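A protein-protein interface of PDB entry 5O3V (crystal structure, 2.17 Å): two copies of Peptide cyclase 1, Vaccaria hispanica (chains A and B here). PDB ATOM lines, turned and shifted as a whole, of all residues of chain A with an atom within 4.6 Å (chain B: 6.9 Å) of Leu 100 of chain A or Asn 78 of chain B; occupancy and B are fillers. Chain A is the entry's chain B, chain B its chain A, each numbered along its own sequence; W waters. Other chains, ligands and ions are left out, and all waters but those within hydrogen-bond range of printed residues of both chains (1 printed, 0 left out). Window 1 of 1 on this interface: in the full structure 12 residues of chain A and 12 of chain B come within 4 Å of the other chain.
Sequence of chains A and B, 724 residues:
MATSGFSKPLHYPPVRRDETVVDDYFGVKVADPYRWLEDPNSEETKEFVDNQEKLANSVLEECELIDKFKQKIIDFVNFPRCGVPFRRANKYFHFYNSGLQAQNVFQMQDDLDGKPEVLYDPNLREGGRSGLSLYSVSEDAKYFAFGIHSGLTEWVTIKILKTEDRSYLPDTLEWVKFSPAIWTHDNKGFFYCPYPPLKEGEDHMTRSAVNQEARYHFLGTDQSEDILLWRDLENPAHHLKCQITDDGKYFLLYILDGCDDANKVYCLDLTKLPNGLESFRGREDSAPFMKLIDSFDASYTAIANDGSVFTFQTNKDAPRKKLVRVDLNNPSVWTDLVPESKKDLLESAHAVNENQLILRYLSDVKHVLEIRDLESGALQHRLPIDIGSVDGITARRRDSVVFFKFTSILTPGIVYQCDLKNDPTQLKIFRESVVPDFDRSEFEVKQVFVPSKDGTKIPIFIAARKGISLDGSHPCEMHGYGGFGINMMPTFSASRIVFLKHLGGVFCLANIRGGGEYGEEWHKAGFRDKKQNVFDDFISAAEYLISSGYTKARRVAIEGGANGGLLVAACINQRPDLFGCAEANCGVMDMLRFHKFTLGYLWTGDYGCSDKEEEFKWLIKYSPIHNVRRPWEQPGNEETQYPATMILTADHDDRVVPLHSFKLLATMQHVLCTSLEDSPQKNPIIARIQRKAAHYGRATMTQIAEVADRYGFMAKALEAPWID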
ATOM      1  N   ILE A  74      13.026 -21.173  17.834  1.00  0.00           N
ATOM      2  CA  ILE A  74      11.575 -20.965  17.681  1.00  0.00           C
ATOM      3  C   ILE A  74      10.828 -22.241  18.069  1.00  0.00           C
ATOM      4  O   ILE A  74       9.887 -22.200  18.867  1.00  0.00           O
ATOM      5  CB  ILE A  74      11.208 -20.496  16.247  1.00  0.00           C
ATOM      6  CG1 ILE A  74      11.645 -19.028  16.060  1.00  0.00           C
ATOM      7  CG2 ILE A  74       9.715 -20.631  15.962  1.00  0.00           C
ATOM      8  CD1 ILE A  74      11.636 -18.553  14.609  1.00  0.00           C
ATOM      9  N   VAL A  77      11.054 -23.135  21.983  1.00  0.00           N
ATOM     10  CA  VAL A  77      10.372 -22.212  22.898  1.00  0.00           C
ATOM     11  C   VAL A  77       8.848 -22.151  22.668  1.00  0.00           C
ATOM     12  O   VAL A  77       8.135 -21.534  23.449  1.00  0.00           O
ATOM     13  CB  VAL A  77      11.056 -20.817  22.875  1.00  0.00           C
ATOM     14  CG1 VAL A  77      10.440 -19.895  21.850  1.00  0.00           C
ATOM     15  CG2 VAL A  77      11.003 -20.182  24.246  1.00  0.00           C
ATOM     16  N   ASN A  78       8.359 -22.842  21.636  1.00  0.00           N
ATOM     17  CA  ASN A  78       6.932 -22.868  21.291  1.00  0.00           C
ATOM     18  C   ASN A  78       6.099 -23.805  22.197  1.00  0.00           C
ATOM     19  O   ASN A  78       5.598 -24.826  21.743  1.00  0.00           O
ATOM     20  CB  ASN A  78       6.759 -23.274  19.802  1.00  0.00           C
ATOM     21  CG  ASN A  78       5.384 -22.908  19.247  1.00  0.00           C
ATOM     22  OD1 ASN A  78       4.595 -22.228  19.911  1.00  0.00           O
ATOM     23  ND2 ASN A  78       5.101 -23.336  18.021  1.00  0.00           N
ATOM     24  N   ASN A  97       1.392 -16.733  28.244  1.00  0.00           N
ATOM     25  CA  ASN A  97       1.880 -16.675  26.864  1.00  0.00           C
ATOM     26  C   ASN A  97       1.597 -18.037  26.215  1.00  0.00           C
ATOM     27  O   ASN A  97       1.956 -19.075  26.782  1.00  0.00           O
ATOM     28  CB  ASN A  97       3.389 -16.373  26.858  1.00  0.00           C
ATOM     29  CG  ASN A  97       3.901 -15.902  25.500  1.00  0.00           C
ATOM     30  OD1 ASN A  97       3.661 -16.539  24.465  1.00  0.00           O
ATOM     31  ND2 ASN A  97       4.644 -14.789  25.506  1.00  0.00           N
ATOM     32  N   SER A  98       0.968 -18.044  25.042  1.00  0.00           N
ATOM     33  CA  SER A  98       0.649 -19.315  24.367  1.00  0.00           C
ATOM     34  C   SER A  98       1.875 -19.961  23.714  1.00  0.00           C
ATOM     35  O   SER A  98       1.753 -21.050  23.147  1.00  0.00           O
ATOM     36  CB  SER A  98      -0.465 -19.130  23.328  1.00  0.00           C
ATOM     37  OG  SER A  98      -0.068 -18.245  22.302  1.00  0.00           O
ATOM     38  N   GLY A  99       3.025 -19.278  23.756  1.00  0.00           N
ATOM     39  CA  GLY A  99       4.304 -19.865  23.364  1.00  0.00           C
ATOM     40  C   GLY A  99       5.197 -18.914  22.591  1.00  0.00           C
ATOM     41  O   GLY A  99       6.384 -18.749  22.929  1.00  0.00           O
ATOM     42  N   LEU A 100       4.630 -18.287  21.561  1.00  0.00           N
ATOM     43  CA  LEU A 100       5.378 -17.390  20.683  1.00  0.00           C
ATOM     44  C   LEU A 100       4.759 -15.994  20.537  1.00  0.00           C
ATOM     45  O   LEU A 100       5.037 -15.302  19.561  1.00  0.00           O
ATOM     46  CB  LEU A 100       5.566 -18.058  19.305  1.00  0.00           C
ATOM     47  CG  LEU A 100       6.509 -19.258  19.269  1.00  0.00           C
ATOM     48  CD1 LEU A 100       6.461 -19.917  17.892  1.00  0.00           C
ATOM     49  CD2 LEU A 100       7.929 -18.855  19.617  1.00  0.00           C
ATOM     50  N   GLN A 101       3.970 -15.568  21.523  1.00  0.00           N
ATOM     51  CA  GLN A 101       3.446 -14.201  21.534  1.00  0.00           C
ATOM     52  C   GLN A 101       4.589 -13.242  21.876  1.00  0.00           C
ATOM     53  O   GLN A 101       5.507 -13.581  22.631  1.00  0.00           O
ATOM     54  CB  GLN A 101       2.294 -14.055  22.525  1.00  0.00           C
ATOM     55  CG  GLN A 101       1.096 -14.968  22.248  1.00  0.00           C
ATOM     56  CD  GLN A 101      -0.038 -14.753  23.236  1.00  0.00           C
ATOM     57  OE1 GLN A 101      -0.144 -15.461  24.248  1.00  0.00           O
ATOM     58  NE2 GLN A 101      -0.880 -13.762  22.965  1.00  0.00           N
ATOM     59  N   ALA A 102       4.532 -12.040  21.298  1.00  0.00           N
ATOM     60  CA  ALA A 102       5.593 -11.045  21.445  1.00  0.00           C
ATOM     61  C   ALA A 102       5.792 -10.637  22.908  1.00  0.00           C
ATOM     62  O   ALA A 102       6.925 -10.437  23.348  1.00  0.00           O
ATOM     63  CB  ALA A 102       5.293  -9.828  20.574  1.00  0.00           C
ATOM     64  N   THR A 700       9.558 -11.253  21.763  1.00  0.00           N
ATOM     65  CA  THR A 700      10.096 -12.620  21.613  1.00  0.00           C
ATOM     66  C   THR A 700      10.949 -12.818  20.339  1.00  0.00           C
ATOM     67  O   THR A 700      12.084 -13.291  20.407  1.00  0.00           O
ATOM     68  CB  THR A 700       8.930 -13.626  21.644  1.00  0.00           C
ATOM     69  OG1 THR A 700       8.248 -13.500  22.895  1.00  0.00           O
ATOM     70  CG2 THR A 700       9.405 -15.082  21.455  1.00  0.00           C
ATOM     71  N   MET A 701      10.416 -12.428  19.185  1.00  0.00           N
ATOM     72  CA  MET A 701      11.133 -12.613  17.918  1.00  0.00           C
ATOM     73  C   MET A 701      12.376 -11.733  17.796  1.00  0.00           C
ATOM     74  O   MET A 701      13.369 -12.134  17.190  1.00  0.00           O
ATOM     75  CB  MET A 701      10.184 -12.407  16.722  1.00  0.00           C
ATOM     76  CG  MET A 701       9.064 -13.446  16.652  1.00  0.00           C
ATOM     77  SD  MET A 701       9.669 -15.122  16.384  1.00  0.00           S
ATOM     78  CE  MET A 701       8.173 -16.058  16.671  1.00  0.00           C
ATOM     79  N   ILE B  73       6.636 -13.591   7.285  1.00  0.00           N
ATOM     80  CA  ILE B  73       5.500 -14.520   7.207  1.00  0.00           C
ATOM     81  C   ILE B  73       5.134 -15.039   8.606  1.00  0.00           C
ATOM     82  O   ILE B  73       3.952 -15.050   8.963  1.00  0.00           O
ATOM     83  CB  ILE B  73       5.771 -15.713   6.260  1.00  0.00           C
ATOM     84  CG1 ILE B  73       5.894 -15.219   4.817  1.00  0.00           C
ATOM     85  CG2 ILE B  73       4.678 -16.772   6.375  1.00  0.00           C
ATOM     86  CD1 ILE B  73       6.584 -16.207   3.899  1.00  0.00           C
ATOM     87  N   ILE B  74       6.141 -15.465   9.380  1.00  0.00           N
ATOM     88  CA  ILE B  74       5.927 -15.908  10.763  1.00  0.00           C
ATOM     89  C   ILE B  74       5.221 -14.804  11.549  1.00  0.00           C
ATOM     90  O   ILE B  74       4.222 -15.061  12.204  1.00  0.00           O
ATOM     91  CB  ILE B  74       7.263 -16.331  11.454  1.00  0.00           C
ATOM     92  CG1 ILE B  74       7.740 -17.676  10.891  1.00  0.00           C
ATOM     93  CG2 ILE B  74       7.122 -16.419  12.976  1.00  0.00           C
ATOM     94  CD1 ILE B  74       9.173 -18.027  11.239  1.00  0.00           C
ATOM     95  N   ASP B  75       5.732 -13.579  11.460  1.00  0.00           N
ATOM     96  CA  ASP B  75       5.158 -12.455  12.198  1.00  0.00           C
ATOM     97  C   ASP B  75       3.700 -12.148  11.762  1.00  0.00           C
ATOM     98  O   ASP B  75       2.816 -12.011  12.613  1.00  0.00           O
ATOM     99  CB  ASP B  75       6.076 -11.204  12.108  1.00  0.00           C
ATOM    100  CG  ASP B  75       7.457 -11.400  12.798  1.00  0.00           C
ATOM    101  OD1 ASP B  75       7.629 -12.352  13.596  1.00  0.00           O
ATOM    102  OD2 ASP B  75       8.377 -10.587  12.549  1.00  0.00           O
ATOM    103  N   PHE B  76       3.440 -12.080  10.459  1.00  0.00           N
ATOM    104  CA  PHE B  76       2.078 -11.786   9.959  1.00  0.00           C
ATOM    105  C   PHE B  76       1.025 -12.880  10.200  1.00  0.00           C
ATOM    106  O   PHE B  76      -0.165 -12.562  10.239  1.00  0.00           O
ATOM    107  CB  PHE B  76       2.088 -11.401   8.473  1.00  0.00           C
ATOM    108  CG  PHE B  76       2.619 -10.007   8.175  1.00  0.00           C
ATOM    109  CD1 PHE B  76       2.804  -9.024   9.166  1.00  0.00           C
ATOM    110  CD2 PHE B  76       2.897  -9.650   6.862  1.00  0.00           C
ATOM    111  CE1 PHE B  76       3.277  -7.758   8.839  1.00  0.00           C
ATOM    112  CE2 PHE B  76       3.372  -8.388   6.544  1.00  0.00           C
ATOM    113  CZ  PHE B  76       3.558  -7.441   7.531  1.00  0.00           C
ATOM    114  N   VAL B  77       1.433 -14.141  10.381  1.00  0.00           N
ATOM    115  CA  VAL B  77       0.479 -15.223  10.636  1.00  0.00           C
ATOM    116  C   VAL B  77       0.321 -15.549  12.141  1.00  0.00           C
ATOM    117  O   VAL B  77      -0.520 -16.370  12.535  1.00  0.00           O
ATOM    118  CB  VAL B  77       0.837 -16.476   9.789  1.00  0.00           C
ATOM    119  CG1 VAL B  77       1.785 -17.435  10.511  1.00  0.00           C
ATOM    120  CG2 VAL B  77      -0.430 -17.195   9.360  1.00  0.00           C
ATOM    121  N   ASN B  78       1.114 -14.890  12.989  1.00  0.00           N
ATOM    122  CA  ASN B  78       1.102 -15.115  14.442  1.00  0.00           C
ATOM    123  C   ASN B  78      -0.056 -14.392  15.139  1.00  0.00           C
ATOM    124  O   ASN B  78       0.152 -13.434  15.877  1.00  0.00           O
ATOM    125  CB  ASN B  78       2.460 -14.692  15.060  1.00  0.00           C
ATOM    126  CG  ASN B  78       2.678 -15.248  16.454  1.00  0.00           C
ATOM    127  OD1 ASN B  78       1.913 -16.083  16.920  1.00  0.00           O
ATOM    128  ND2 ASN B  78       3.739 -14.790  17.126  1.00  0.00           N
ATOM    129  N   PHE B  79      -1.273 -14.881  14.900  1.00  0.00           N
ATOM    130  CA  PHE B  79      -2.480 -14.404  15.585  1.00  0.00           C
ATOM    131  C   PHE B  79      -3.381 -15.618  15.836  1.00  0.00           C
ATOM    132  O   PHE B  79      -3.385 -16.550  15.028  1.00  0.00           O
ATOM    133  CB  PHE B  79      -3.244 -13.349  14.757  1.00  0.00           C
ATOM    134  CG  PHE B  79      -3.589 -13.796  13.357  1.00  0.00           C
ATOM    135  CD1 PHE B  79      -2.721 -13.528  12.316  1.00  0.00           C
ATOM    136  CD2 PHE B  79      -4.786 -14.461  13.065  1.00  0.00           C
ATOM    137  CE1 PHE B  79      -3.022 -13.926  11.011  1.00  0.00           C
ATOM    138  CE2 PHE B  79      -5.086 -14.865  11.771  1.00  0.00           C
ATOM    139  CZ  PHE B  79      -4.201 -14.602  10.745  1.00  0.00           C
ATOM    140  N   PRO B  80      -4.174 -15.601  16.929  1.00  0.00           N
ATOM    141  CA  PRO B  80      -5.054 -16.744  17.193  1.00  0.00           C
ATOM    142  C   PRO B  80      -6.214 -16.887  16.191  1.00  0.00           C
ATOM    143  O   PRO B  80      -6.759 -15.882  15.737  1.00  0.00           O
ATOM    144  CB  PRO B  80      -5.575 -16.462  18.610  1.00  0.00           C
ATOM    145  CG  PRO B  80      -5.473 -14.989  18.761  1.00  0.00           C
ATOM    146  CD  PRO B  80      -4.245 -14.595  18.006  1.00  0.00           C
ATOM    147  N   ARG B  81      -6.576 -18.132  15.870  1.00  0.00           N
ATOM    148  CA  ARG B  81      -7.611 -18.455  14.872  1.00  0.00           C
ATOM    149  C   ARG B  81      -8.652 -19.411  15.452  1.00  0.00           C
ATOM    150  O   ARG B  81      -8.338 -20.591  15.730  1.00  0.00           O
ATOM    151  CB  ARG B  81      -6.973 -19.104  13.640  1.00  0.00           C
ATOM    152  CG  ARG B  81      -6.179 -18.137  12.763  1.00  0.00           C
ATOM    153  CD  ARG B  81      -5.565 -18.824  11.542  1.00  0.00           C
ATOM    154  NE  ARG B  81      -4.529 -19.815  11.885  1.00  0.00           N
ATOM    155  CZ  ARG B  81      -3.277 -19.539  12.260  1.00  0.00           C
ATOM    156  NH1 ARG B  81      -2.838 -18.284  12.374  1.00  0.00           N
ATOM    157  NH2 ARG B  81      -2.440 -20.539  12.543  1.00  0.00           N
ATOM    158  N   SER B  98      -3.420 -21.306  18.391  1.00  0.00           N
ATOM    159  CA  SER B  98      -2.971 -20.091  19.088  1.00  0.00           C
ATOM    160  C   SER B  98      -2.111 -19.175  18.208  1.00  0.00           C
ATOM    161  O   SER B  98      -1.703 -18.106  18.649  1.00  0.00           O
ATOM    162  CB  SER B  98      -2.227 -20.437  20.381  1.00  0.00           C
ATOM    163  OG  SER B  98      -1.052 -21.175  20.101  1.00  0.00           O
ATOM    164  N   GLY B  99      -1.813 -19.610  16.980  1.00  0.00           N
ATOM    165  CA  GLY B  99      -1.184 -18.763  15.958  1.00  0.00           C
ATOM    166  C   GLY B  99      -0.126 -19.487  15.155  1.00  0.00           C
ATOM    167  O   GLY B  99      -0.136 -19.432  13.918  1.00  0.00           O
ATOM    168  N   LEU B 100       0.786 -20.170  15.859  1.00  0.00           N
ATOM    169  CA  LEU B 100       1.912 -20.850  15.245  1.00  0.00           C
ATOM    170  C   LEU B 100       2.039 -22.328  15.672  1.00  0.00           C
ATOM    171  O   LEU B 100       3.128 -22.902  15.604  1.00  0.00           O
ATOM    172  CB  LEU B 100       3.207 -20.072  15.553  1.00  0.00           C
ATOM    173  CG  LEU B 100       3.336 -18.681  14.894  1.00  0.00           C
ATOM    174  CD1 LEU B 100       4.561 -17.952  15.408  1.00  0.00           C
ATOM    175  CD2 LEU B 100       3.406 -18.773  13.377  1.00  0.00           C
ATOM    176  N   GLN B 101       0.944 -22.955  16.093  1.00  0.00           N
ATOM    177  CA  GLN B 101       0.950 -24.401  16.350  1.00  0.00           C
ATOM    178  C   GLN B 101       1.027 -25.163  15.021  1.00  0.00           C
ATOM    179  O   GLN B 101       0.492 -24.693  13.999  1.00  0.00           O
ATOM    180  CB  GLN B 101      -0.288 -24.838  17.139  1.00  0.00           C
ATOM    181  CG  GLN B 101      -0.426 -24.173  18.501  1.00  0.00           C
ATOM    182  CD  GLN B 101      -1.654 -24.649  19.263  1.00  0.00           C
ATOM    183  OE1 GLN B 101      -2.707 -24.014  19.215  1.00  0.00           O
ATOM    184  NE2 GLN B 101      -1.534 -25.779  19.947  1.00  0.00           N
ATOM    185  N   VAL B 434      -6.785 -10.467  13.854  1.00  0.00           N
ATOM    186  CA  VAL B 434      -6.088  -9.224  13.492  1.00  0.00           C
ATOM    187  C   VAL B 434      -4.629  -9.536  13.126  1.00  0.00           C
ATOM    188  O   VAL B 434      -3.944 -10.281  13.861  1.00  0.00           O
ATOM    189  CB  VAL B 434      -6.128  -8.194  14.647  1.00  0.00           C
ATOM    190  CG1 VAL B 434      -5.424  -6.890  14.263  1.00  0.00           C
ATOM    191  CG2 VAL B 434      -7.572  -7.915  15.069  1.00  0.00           C
ATOM    192  N   VAL B 435      -4.169  -8.976  11.998  1.00  0.00           N
ATOM    193  CA  VAL B 435      -2.775  -9.108  11.561  1.00  0.00           C
ATOM    194  C   VAL B 435      -1.929  -8.118  12.380  1.00  0.00           C
ATOM    195  O   VAL B 435      -2.204  -6.919  12.338  1.00  0.00           O
ATOM    196  CB  VAL B 435      -2.583  -8.797  10.053  1.00  0.00           C
ATOM    197  CG1 VAL B 435      -1.125  -9.009   9.634  1.00  0.00           C
ATOM    198  CG2 VAL B 435      -3.504  -9.636   9.182  1.00  0.00           C
ATOM    199  N   PRO B 436      -0.897  -8.613  13.120  1.00  0.00           N
ATOM    200  CA  PRO B 436      -0.072  -7.709  13.929  1.00  0.00           C
ATOM    201  C   PRO B 436       0.789  -6.753  13.100  1.00  0.00           C
ATOM    202  O   PRO B 436       1.473  -7.191  12.180  1.00  0.00           O
ATOM    203  CB  PRO B 436       0.829  -8.659  14.744  1.00  0.00           C
ATOM    204  CG  PRO B 436       0.323 -10.030  14.509  1.00  0.00           C
ATOM    205  CD  PRO B 436      -0.423 -10.006  13.214  1.00  0.00           C
ATOM    206  N   ALA B 494      -1.054 -14.696   4.301  1.00  0.00           N
ATOM    207  CA  ALA B 494      -0.088 -13.859   5.013  1.00  0.00           C
ATOM    208  C   ALA B 494       1.103 -13.528   4.118  1.00  0.00           C
ATOM    209  O   ALA B 494       1.558 -12.379   4.100  1.00  0.00           O
ATOM    210  CB  ALA B 494       0.364 -14.521   6.294  1.00  0.00           C
ATOM    211  N   MET B 701       5.227 -24.668  10.152  1.00  0.00           N
ATOM    212  CA  MET B 701       6.615 -24.280   9.843  1.00  0.00           C
ATOM    213  C   MET B 701       7.129 -24.902   8.531  1.00  0.00           C
ATOM    214  O   MET B 701       7.923 -24.282   7.819  1.00  0.00           O
ATOM    215  CB  MET B 701       7.562 -24.608  11.005  1.00  0.00           C
ATOM    216  CG  MET B 701       7.285 -23.818  12.273  1.00  0.00           C
ATOM    217  SD  MET B 701       7.429 -22.015  12.108  1.00  0.00           S
ATOM    218  CE  MET B 701       6.922 -21.555  13.762  1.00  0.00           C
HETATM  219  O   HOH W   1      -0.032 -22.646  22.115  1.00  0.00           O
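Of the 11 printed residues of chain A, 5 touch a printed residue of chain B. Of the 18 printed residues of chain B, 6 touch a printed residue of chain A. Hydrophobic or aromatic side chains of chain B that line the printed part of chain A: Ile 74, Leu 100 and Met 701. Among the printed residues, 7 pairs touch across the chains.
Of chain A, only Leu 100 (2.8 Å) comes within 4 Å of Asn 78 of chain B. Printed residues of chain A within 4 Å of Ile 74 of chain B: Met 701 (3.9 Å). Of the printed residues of chain A, Asp 75 of chain B touches Met 701. Of the printed residues of chain A, Met 701 of chain B touches Ile 74 (3.7 Å). Printed residues of chain B within 4 Å of Ser 98 of chain A: Ser 98. Ala 102 of chain A touches none of the printed residues of chain B. Val 77 of chain A touches none of the printed residues of chain B. The nearest residue of chain A that does not touch Asn 78 of chain B is Gln 101 of chain A (4.5 Å).
The backbone NH (N) of Ser 98 of chain B lies within hydrogen-bond range of the side-chain amide oxygen (OE1) of Gln 101 of chain B (2.9 Å). OE1 of Gln 101 of chain A sits at hydrogen-bond distance from N of Ser 98 of chain A (2.9 Å).
The side-chain amide nitrogen (ND2) of Asn 78 of chain B sits at hydrogen-bond distance from the backbone carbonyl oxygen (O) of Leu 100 of chain A. The backbone carbonyl oxygen (O) of Leu 100 of chain B sits at hydrogen-bond distance from the side-chain amide nitrogen (ND2) of Asn 78 of chain A (3.2 Å).
Ile 74 of chain A touches Met 701 of chain B, and with the chains exchanged Met 701 of chain A touches Ile 74 of chain B. Asn 78 of chain A touches Leu 100 of chain B, and with the chains exchanged Leu 100 of chain A touches Asn 78 of chain B. Ser 98 of chain A touches its own counterpart, Ser 98 of chain B. Leu 100 of chain B touches its own counterpart, Leu 100 of chain A. Positions printed for both chains: 74, 77, 78, 98, 99, 100, 101 and 701. Of the 7 pairs that touch across the chains among the printed residues, 6 have their exchanged pair printed and touching as well.
Water W1 bridges the backbone carbonyl oxygen (O) of Ser 98 of chain A (2.6 Å) and the side-chain hydroxyl (OG) of Ser 98 of chain B (2.7 Å).
Met 701 of chain B touches Ile 74 of chain A. Ser 98 of chain A touches Ser 98 of chain B (OG to CB, 3.6 Å). Leu 100 of chain A touches Leu 100 of chain B (CD1 to CD1, 3.7 Å). Met 701 of chain A touches Ile 74 of chain B. CG of Met 701 of chain A touches OD1 of Asp 75 of chain B, at 3.5 Å.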
